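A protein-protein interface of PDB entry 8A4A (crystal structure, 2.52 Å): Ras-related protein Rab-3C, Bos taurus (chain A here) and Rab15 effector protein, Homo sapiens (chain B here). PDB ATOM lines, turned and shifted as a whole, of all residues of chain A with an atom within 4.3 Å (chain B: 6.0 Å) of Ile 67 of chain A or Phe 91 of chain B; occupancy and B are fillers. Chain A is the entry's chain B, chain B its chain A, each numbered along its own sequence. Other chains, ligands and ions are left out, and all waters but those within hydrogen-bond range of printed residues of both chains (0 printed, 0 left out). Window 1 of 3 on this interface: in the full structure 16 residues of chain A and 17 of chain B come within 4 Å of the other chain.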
ATOM      1  N   VAL A  65      18.176 -19.449  16.490  1.00  0.00           N
ATOM      2  CA  VAL A  65      17.347 -19.232  17.667  1.00  0.00           C
ATOM      3  C   VAL A  65      18.272 -19.210  18.873  1.00  0.00           C
ATOM      4  O   VAL A  65      18.877 -20.228  19.225  1.00  0.00           O
ATOM      5  CB  VAL A  65      16.270 -20.312  17.812  1.00  0.00           C
ATOM      6  CG1 VAL A  65      15.421 -20.042  19.048  1.00  0.00           C
ATOM      7  CG2 VAL A  65      15.402 -20.361  16.563  1.00  0.00           C
ATOM      8  N   GLY A  66      18.411 -18.042  19.493  1.00  0.00           N
ATOM      9  CA  GLY A  66      19.198 -17.965  20.703  1.00  0.00           C
ATOM     10  C   GLY A  66      20.674 -17.854  20.399  1.00  0.00           C
ATOM     11  O   GLY A  66      21.185 -16.781  20.072  1.00  0.00           O
ATOM     12  N   ILE A  67      21.371 -18.980  20.511  1.00  0.00           N
ATOM     13  CA  ILE A  67      22.817 -19.013  20.347  1.00  0.00           C
ATOM     14  C   ILE A  67      23.205 -20.463  20.104  1.00  0.00           C
ATOM     15  O   ILE A  67      22.434 -21.382  20.382  1.00  0.00           O
ATOM     16  CB  ILE A  67      23.523 -18.414  21.592  1.00  0.00           C
ATOM     17  CG1 ILE A  67      24.898 -17.852  21.226  1.00  0.00           C
ATOM     18  CG2 ILE A  67      23.619 -19.446  22.714  1.00  0.00           C
ATOM     19  CD1 ILE A  67      25.661 -17.306  22.406  1.00  0.00           C
ATOM     20  N   ASP A  68      24.390 -20.672  19.542  1.00  0.00           N
ATOM     21  CA  ASP A  68      24.935 -22.023  19.424  1.00  0.00           C
ATOM     22  C   ASP A  68      26.452 -21.899  19.404  1.00  0.00           C
ATOM     23  O   ASP A  68      26.991 -20.794  19.434  1.00  0.00           O
ATOM     24  CB  ASP A  68      24.375 -22.743  18.188  1.00  0.00           C
ATOM     25  CG  ASP A  68      24.439 -24.265  18.311  1.00  0.00           C
ATOM     26  OD1 ASP A  68      25.311 -24.773  19.044  1.00  0.00           O
ATOM     27  OD2 ASP A  68      23.623 -24.954  17.661  1.00  0.00           O
ATOM     28  N   TRP A  86      31.148 -19.078  19.438  1.00  0.00           N
ATOM     29  CA  TRP A  86      29.721 -18.939  19.669  1.00  0.00           C
ATOM     30  C   TRP A  86      29.113 -18.102  18.556  1.00  0.00           C
ATOM     31  O   TRP A  86      29.641 -17.043  18.213  1.00  0.00           O
ATOM     32  CB  TRP A  86      29.458 -18.277  21.019  1.00  0.00           C
ATOM     33  CG  TRP A  86      29.939 -19.080  22.177  1.00  0.00           C
ATOM     34  CD1 TRP A  86      31.224 -19.188  22.629  1.00  0.00           C
ATOM     35  CD2 TRP A  86      29.139 -19.893  23.036  1.00  0.00           C
ATOM     36  NE1 TRP A  86      31.270 -20.021  23.722  1.00  0.00           N
ATOM     37  CE2 TRP A  86      30.002 -20.468  23.991  1.00  0.00           C
ATOM     38  CE3 TRP A  86      27.775 -20.192  23.092  1.00  0.00           C
ATOM     39  CZ2 TRP A  86      29.545 -21.322  24.986  1.00  0.00           C
ATOM     40  CZ3 TRP A  86      27.323 -21.040  24.085  1.00  0.00           C
ATOM     41  CH2 TRP A  86      28.205 -21.594  25.018  1.00  0.00           C
ATOM     42  N   ASP A  87      28.016 -18.592  17.997  1.00  0.00           N
ATOM     43  CA  ASP A  87      27.257 -17.950  16.933  1.00  0.00           C
ATOM     44  C   ASP A  87      26.000 -17.378  17.577  1.00  0.00           C
ATOM     45  O   ASP A  87      25.156 -18.144  18.068  1.00  0.00           O
ATOM     46  CB  ASP A  87      26.945 -18.986  15.851  1.00  0.00           C
ATOM     47  CG  ASP A  87      25.948 -18.499  14.816  1.00  0.00           C
ATOM     48  OD1 ASP A  87      26.000 -17.309  14.431  1.00  0.00           O
ATOM     49  OD2 ASP A  87      25.118 -19.332  14.374  1.00  0.00           O
ATOM     50  N   THR A  88      25.878 -16.044  17.614  1.00  0.00           N
ATOM     51  CA  THR A  88      24.744 -15.443  18.303  1.00  0.00           C
ATOM     52  C   THR A  88      23.614 -15.127  17.331  1.00  0.00           C
ATOM     53  O   THR A  88      23.816 -14.994  16.120  1.00  0.00           O
ATOM     54  CB  THR A  88      25.160 -14.166  19.042  1.00  0.00           C
ATOM     55  OG1 THR A  88      25.568 -13.168  18.098  1.00  0.00           O
ATOM     56  CG2 THR A  88      26.303 -14.454  20.010  1.00  0.00           C
ATOM     57  N   ILE A  97      19.421 -12.985  25.866  1.00  0.00           N
ATOM     58  CA  ILE A  97      20.100 -14.268  25.971  1.00  0.00           C
ATOM     59  C   ILE A  97      21.509 -14.175  25.391  1.00  0.00           C
ATOM     60  O   ILE A  97      22.474 -14.657  26.003  1.00  0.00           O
ATOM     61  CB  ILE A  97      19.263 -15.390  25.325  1.00  0.00           C
ATOM     62  CG1 ILE A  97      19.988 -16.729  25.446  1.00  0.00           C
ATOM     63  CG2 ILE A  97      18.913 -15.077  23.874  1.00  0.00           C
ATOM     64  CD1 ILE A  97      19.063 -17.885  25.712  1.00  0.00           C
ATOM     65  N   TYR A 101      25.650 -14.566  27.254  1.00  0.00           N
ATOM     66  CA  TYR A 101      26.744 -15.465  26.919  1.00  0.00           C
ATOM     67  C   TYR A 101      28.027 -14.731  26.541  1.00  0.00           C
ATOM     68  O   TYR A 101      29.001 -15.381  26.143  1.00  0.00           O
ATOM     69  CB  TYR A 101      26.309 -16.410  25.793  1.00  0.00           C
ATOM     70  CG  TYR A 101      25.416 -17.535  26.279  1.00  0.00           C
ATOM     71  CD1 TYR A 101      24.060 -17.326  26.505  1.00  0.00           C
ATOM     72  CD2 TYR A 101      25.929 -18.804  26.512  1.00  0.00           C
ATOM     73  CE1 TYR A 101      23.244 -18.351  26.956  1.00  0.00           C
ATOM     74  CE2 TYR A 101      25.121 -19.834  26.956  1.00  0.00           C
ATOM     75  CZ  TYR A 101      23.780 -19.602  27.176  1.00  0.00           C
ATOM     76  OH  TYR A 101      22.973 -20.628  27.622  1.00  0.00           O
ATOM     77  N   MET B  83      16.236 -28.323  18.540  1.00  0.00           N
ATOM     78  CA  MET B  83      17.500 -27.901  19.113  1.00  0.00           C
ATOM     79  C   MET B  83      18.600 -28.859  18.687  1.00  0.00           C
ATOM     80  O   MET B  83      18.388 -30.074  18.599  1.00  0.00           O
ATOM     81  CB  MET B  83      17.403 -27.852  20.640  1.00  0.00           C
ATOM     82  CG  MET B  83      16.319 -26.913  21.209  1.00  0.00           C
ATOM     83  SD  MET B  83      16.546 -25.124  21.073  1.00  0.00           S
ATOM     84  CE  MET B  83      16.292 -24.762  19.334  1.00  0.00           C
ATOM     85  N   HIS B  86      24.077 -29.307  21.304  1.00  0.00           N
ATOM     86  CA  HIS B  86      24.590 -28.225  22.136  1.00  0.00           C
ATOM     87  C   HIS B  86      23.457 -27.354  22.659  1.00  0.00           C
ATOM     88  O   HIS B  86      23.446 -26.970  23.835  1.00  0.00           O
ATOM     89  CB  HIS B  86      25.583 -27.385  21.334  1.00  0.00           C
ATOM     90  CG  HIS B  86      26.892 -28.068  21.087  1.00  0.00           C
ATOM     91  ND1 HIS B  86      27.791 -27.629  20.139  1.00  0.00           N
ATOM     92  CD2 HIS B  86      27.450 -29.163  21.656  1.00  0.00           C
ATOM     93  CE1 HIS B  86      28.849 -28.421  20.138  1.00  0.00           C
ATOM     94  NE2 HIS B  86      28.667 -29.359  21.049  1.00  0.00           N
ATOM     95  N   GLN B  87      22.492 -27.028  21.798  1.00  0.00           N
ATOM     96  CA  GLN B  87      21.385 -26.185  22.231  1.00  0.00           C
ATOM     97  C   GLN B  87      20.499 -26.901  23.239  1.00  0.00           C
ATOM     98  O   GLN B  87      20.045 -26.293  24.213  1.00  0.00           O
ATOM     99  CB  GLN B  87      20.568 -25.726  21.029  1.00  0.00           C
ATOM    100  CG  GLN B  87      21.169 -24.551  20.306  1.00  0.00           C
ATOM    101  CD  GLN B  87      20.431 -24.239  19.023  1.00  0.00           C
ATOM    102  OE1 GLN B  87      19.795 -25.116  18.434  1.00  0.00           O
ATOM    103  NE2 GLN B  87      20.484 -22.979  18.599  1.00  0.00           N
ATOM    104  N   ALA B  88      20.228 -28.189  23.023  1.00  0.00           N
ATOM    105  CA  ALA B  88      19.432 -28.929  23.996  1.00  0.00           C
ATOM    106  C   ALA B  88      20.117 -28.948  25.355  1.00  0.00           C
ATOM    107  O   ALA B  88      19.460 -28.792  26.392  1.00  0.00           O
ATOM    108  CB  ALA B  88      19.169 -30.349  23.497  1.00  0.00           C
ATOM    109  N   PHE B  89      21.442 -29.117  25.371  1.00  0.00           N
ATOM    110  CA  PHE B  89      22.172 -29.042  26.631  1.00  0.00           C
ATOM    111  C   PHE B  89      22.046 -27.661  27.268  1.00  0.00           C
ATOM    112  O   PHE B  89      21.673 -27.540  28.440  1.00  0.00           O
ATOM    113  CB  PHE B  89      23.643 -29.393  26.409  1.00  0.00           C
ATOM    114  CG  PHE B  89      24.446 -29.412  27.672  1.00  0.00           C
ATOM    115  CD1 PHE B  89      24.393 -30.501  28.522  1.00  0.00           C
ATOM    116  CD2 PHE B  89      25.241 -28.334  28.019  1.00  0.00           C
ATOM    117  CE1 PHE B  89      25.121 -30.520  29.692  1.00  0.00           C
ATOM    118  CE2 PHE B  89      25.973 -28.346  29.188  1.00  0.00           C
ATOM    119  CZ  PHE B  89      25.914 -29.441  30.026  1.00  0.00           C
ATOM    120  N   LEU B  90      22.342 -26.604  26.506  1.00  0.00           N
ATOM    121  CA  LEU B  90      22.406 -25.262  27.087  1.00  0.00           C
ATOM    122  C   LEU B  90      21.041 -24.782  27.565  1.00  0.00           C
ATOM    123  O   LEU B  90      20.935 -24.153  28.624  1.00  0.00           O
ATOM    124  CB  LEU B  90      22.972 -24.273  26.069  1.00  0.00           C
ATOM    125  CG  LEU B  90      24.477 -24.316  25.817  1.00  0.00           C
ATOM    126  CD1 LEU B  90      24.791 -23.566  24.544  1.00  0.00           C
ATOM    127  CD2 LEU B  90      25.246 -23.734  26.989  1.00  0.00           C
ATOM    128  N   PHE B  91      19.991 -25.047  26.791  1.00  0.00           N
ATOM    129  CA  PHE B  91      18.684 -24.455  27.036  1.00  0.00           C
ATOM    130  C   PHE B  91      17.752 -25.337  27.849  1.00  0.00           C
ATOM    131  O   PHE B  91      16.731 -24.842  28.335  1.00  0.00           O
ATOM    132  CB  PHE B  91      17.992 -24.125  25.709  1.00  0.00           C
ATOM    133  CG  PHE B  91      18.794 -23.227  24.806  1.00  0.00           C
ATOM    134  CD1 PHE B  91      19.750 -22.364  25.323  1.00  0.00           C
ATOM    135  CD2 PHE B  91      18.581 -23.242  23.435  1.00  0.00           C
ATOM    136  CE1 PHE B  91      20.481 -21.536  24.489  1.00  0.00           C
ATOM    137  CE2 PHE B  91      19.310 -22.422  22.597  1.00  0.00           C
ATOM    138  CZ  PHE B  91      20.260 -21.564  23.123  1.00  0.00           C
ATOM    139  N   GLY B  92      18.065 -26.621  28.003  1.00  0.00           N
ATOM    140  CA  GLY B  92      17.111 -27.518  28.619  1.00  0.00           C
ATOM    141  C   GLY B  92      15.836 -27.704  27.829  1.00  0.00           C
ATOM    142  O   GLY B  92      14.812 -28.083  28.400  1.00  0.00           O
ATOM    143  N   ALA B  93      15.864 -27.435  26.527  1.00  0.00           N
ATOM    144  CA  ALA B  93      14.699 -27.591  25.673  1.00  0.00           C
ATOM    145  C   ALA B  93      15.059 -28.487  24.501  1.00  0.00           C
ATOM    146  O   ALA B  93      16.179 -28.433  23.983  1.00  0.00           O
ATOM    147  CB  ALA B  93      14.191 -26.239  25.167  1.00  0.00           C
ATOM    148  N   ILE B  96      11.413 -25.964  19.975  1.00  0.00           N
ATOM    149  CA  ILE B  96      10.719 -24.703  20.211  1.00  0.00           C
ATOM    150  C   ILE B  96       9.692 -24.498  19.108  1.00  0.00           C
ATOM    151  O   ILE B  96      10.002 -24.651  17.922  1.00  0.00           O
ATOM    152  CB  ILE B  96      11.698 -23.515  20.278  1.00  0.00           C
ATOM    153  CG1 ILE B  96      12.640 -23.680  21.474  1.00  0.00           C
ATOM    154  CG2 ILE B  96      10.941 -22.199  20.375  1.00  0.00           C
ATOM    155  CD1 ILE B  96      13.812 -22.737  21.461  1.00  0.00           C
ATOM    156  N   ARG B 146      18.286 -29.905  33.924  1.00  0.00           N
ATOM    157  CA  ARG B 146      17.511 -29.546  32.740  1.00  0.00           C
ATOM    158  C   ARG B 146      16.372 -28.602  33.097  1.00  0.00           C
ATOM    159  O   ARG B 146      16.114 -27.625  32.380  1.00  0.00           O
ATOM    160  CB  ARG B 146      16.959 -30.805  32.069  1.00  0.00           C
ATOM    161  CG  ARG B 146      18.003 -31.702  31.417  1.00  0.00           C
ATOM    162  CD  ARG B 146      17.458 -32.342  30.145  1.00  0.00           C
ATOM    163  NE  ARG B 146      17.561 -31.466  28.983  1.00  0.00           N
ATOM    164  CZ  ARG B 146      16.826 -31.589  27.885  1.00  0.00           C
ATOM    165  NH1 ARG B 146      15.892 -32.522  27.781  1.00  0.00           N
ATOM    166  NH2 ARG B 146      17.035 -30.757  26.866  1.00  0.00           N
ATOM    167  N   LYS B 149      17.717 -25.072  33.693  1.00  0.00           N
ATOM    168  CA  LYS B 149      18.169 -24.479  32.440  1.00  0.00           C
ATOM    169  C   LYS B 149      16.990 -24.051  31.570  1.00  0.00           C
ATOM    170  O   LYS B 149      17.035 -22.987  30.945  1.00  0.00           O
ATOM    171  CB  LYS B 149      19.092 -25.450  31.706  1.00  0.00           C
ATOM    172  CG  LYS B 149      20.465 -25.548  32.367  1.00  0.00           C
ATOM    173  CD  LYS B 149      21.458 -26.351  31.556  1.00  0.00           C
ATOM    174  CE  LYS B 149      21.109 -27.827  31.558  1.00  0.00           C
ATOM    175  NZ  LYS B 149      22.274 -28.651  31.130  1.00  0.00           N
ATOM    176  N   LEU B 150      15.919 -24.853  31.528  1.00  0.00           N
ATOM    177  CA  LEU B 150      14.712 -24.418  30.827  1.00  0.00           C
ATOM    178  C   LEU B 150      14.120 -23.172  31.471  1.00  0.00           C
ATOM    179  O   LEU B 150      13.681 -22.248  30.771  1.00  0.00           O
ATOM    180  CB  LEU B 150      13.668 -25.535  30.794  1.00  0.00           C
ATOM    181  CG  LEU B 150      12.412 -25.169  29.993  1.00  0.00           C
ATOM    182  CD1 LEU B 150      12.754 -24.898  28.525  1.00  0.00           C
ATOM    183  CD2 LEU B 150      11.347 -26.245  30.101  1.00  0.00           C
ATOM    184  N   GLU B 151      14.087 -23.135  32.804  1.00  0.00           N
ATOM    185  CA  GLU B 151      13.579 -21.953  33.492  1.00  0.00           C
ATOM    186  C   GLU B 151      14.390 -20.715  33.121  1.00  0.00           C
ATOM    187  O   GLU B 151      13.828 -19.661  32.803  1.00  0.00           O
ATOM    188  CB  GLU B 151      13.594 -22.181  35.004  1.00  0.00           C
ATOM    189  CG  GLU B 151      12.741 -21.194  35.786  1.00  0.00           C
ATOM    190  CD  GLU B 151      12.908 -21.340  37.289  1.00  0.00           C
ATOM    191  OE1 GLU B 151      13.673 -22.230  37.722  1.00  0.00           O
ATOM    192  OE2 GLU B 151      12.267 -20.576  38.040  1.00  0.00           O
ATOM    193  N   PHE B 153      16.282 -20.263  30.446  1.00  0.00           N
ATOM    194  CA  PHE B 153      16.060 -19.960  29.037  1.00  0.00           C
ATOM    195  C   PHE B 153      14.779 -19.158  28.851  1.00  0.00           C
ATOM    196  O   PHE B 153      14.770 -18.119  28.176  1.00  0.00           O
ATOM    197  CB  PHE B 153      16.009 -21.266  28.241  1.00  0.00           C
ATOM    198  CG  PHE B 153      15.823 -21.075  26.767  1.00  0.00           C
ATOM    199  CD1 PHE B 153      16.875 -20.663  25.966  1.00  0.00           C
ATOM    200  CD2 PHE B 153      14.587 -21.298  26.182  1.00  0.00           C
ATOM    201  CE1 PHE B 153      16.702 -20.485  24.603  1.00  0.00           C
ATOM    202  CE2 PHE B 153      14.402 -21.115  24.822  1.00  0.00           C
ATOM    203  CZ  PHE B 153      15.462 -20.708  24.028  1.00  0.00           C
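Among the printed residues, pairs that only touch across the chains: Asp 68 of chain A with His 86 of chain B, Ile 67 of chain A with Phe 91 of chain B, Asp 68 of chain A with Gln 87 of chain B, Ile 97 of chain A with Phe 153 of chain B, Trp 86 of chain A with Leu 90 of chain B, Tyr 101 of chain A with Leu 90 of chain B and Val 65 of chain A with Ile 96 of chain B.
Of the 9 printed residues of chain A, 6 touch a printed residue of chain B.
Printed residues of chain A that touch a printed residue of chain B: Val 65, Ile 67, Asp 68, Trp 86, Ile 97 and Tyr 101.
Hydrophobic or aromatic side chains of chain A within 4 Å of the printed part of chain B: Val 65, Ile 67, Trp 86, Ile 97 and Tyr 101.
Of the 15 printed residues of chain B, 6 touch a printed residue of chain A.
Printed residues of chain B that touch a printed residue of chain A: His 86, Gln 87, Leu 90, Phe 91, Ile 96 and Phe 153.
Hydrophobic or aromatic side chains of chain B that line the printed part of chain A: His 86, Leu 90, Phe 91, Ile 96 and Phe 153.
Among the printed residues, no Asp or Glu carboxylate lies within 4 Å of a Lys or Arg side-chain nitrogen of the other chain.
NE2 of Gln 87 of chain B lies within hydrogen-bond range of O of Val 65 of chain A (3.2 Å).
The side-chain amide nitrogen of Gln 87 of chain B lies within hydrogen-bond range of the backbone carbonyl oxygen of Ile 67 of chain A, at 3.1 Å.
The backbone carbonyl oxygen (O) of Phe 91 of chain B sits close to the backbone NH (N) of Leu 150 of chain B (3.3 Å).
N of Asp 87 of chain A lies within hydrogen-bond range of O of Asp 68 of chain A.
Printed residues of chain B within 4 Å of Ile 67 of chain A: Gln 87 (3.1 Å) and Phe 91 (3.5 Å).
Phe 91 of chain B touches one residue of chain A.
Printed residues of chain A within 4 Å of Phe 153 of chain B: Ile 97 (3.5 Å).
Of the printed residues of chain B, Tyr 101 of chain A touches Leu 90.
Printed residues of chain A within 4 Å of Ile 96 of chain B: Val 65 (3.96 Å).
The nearest printed residue of chain A that does not touch Gln 87 of chain B is Gly 66 of chain A (5.4 Å).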
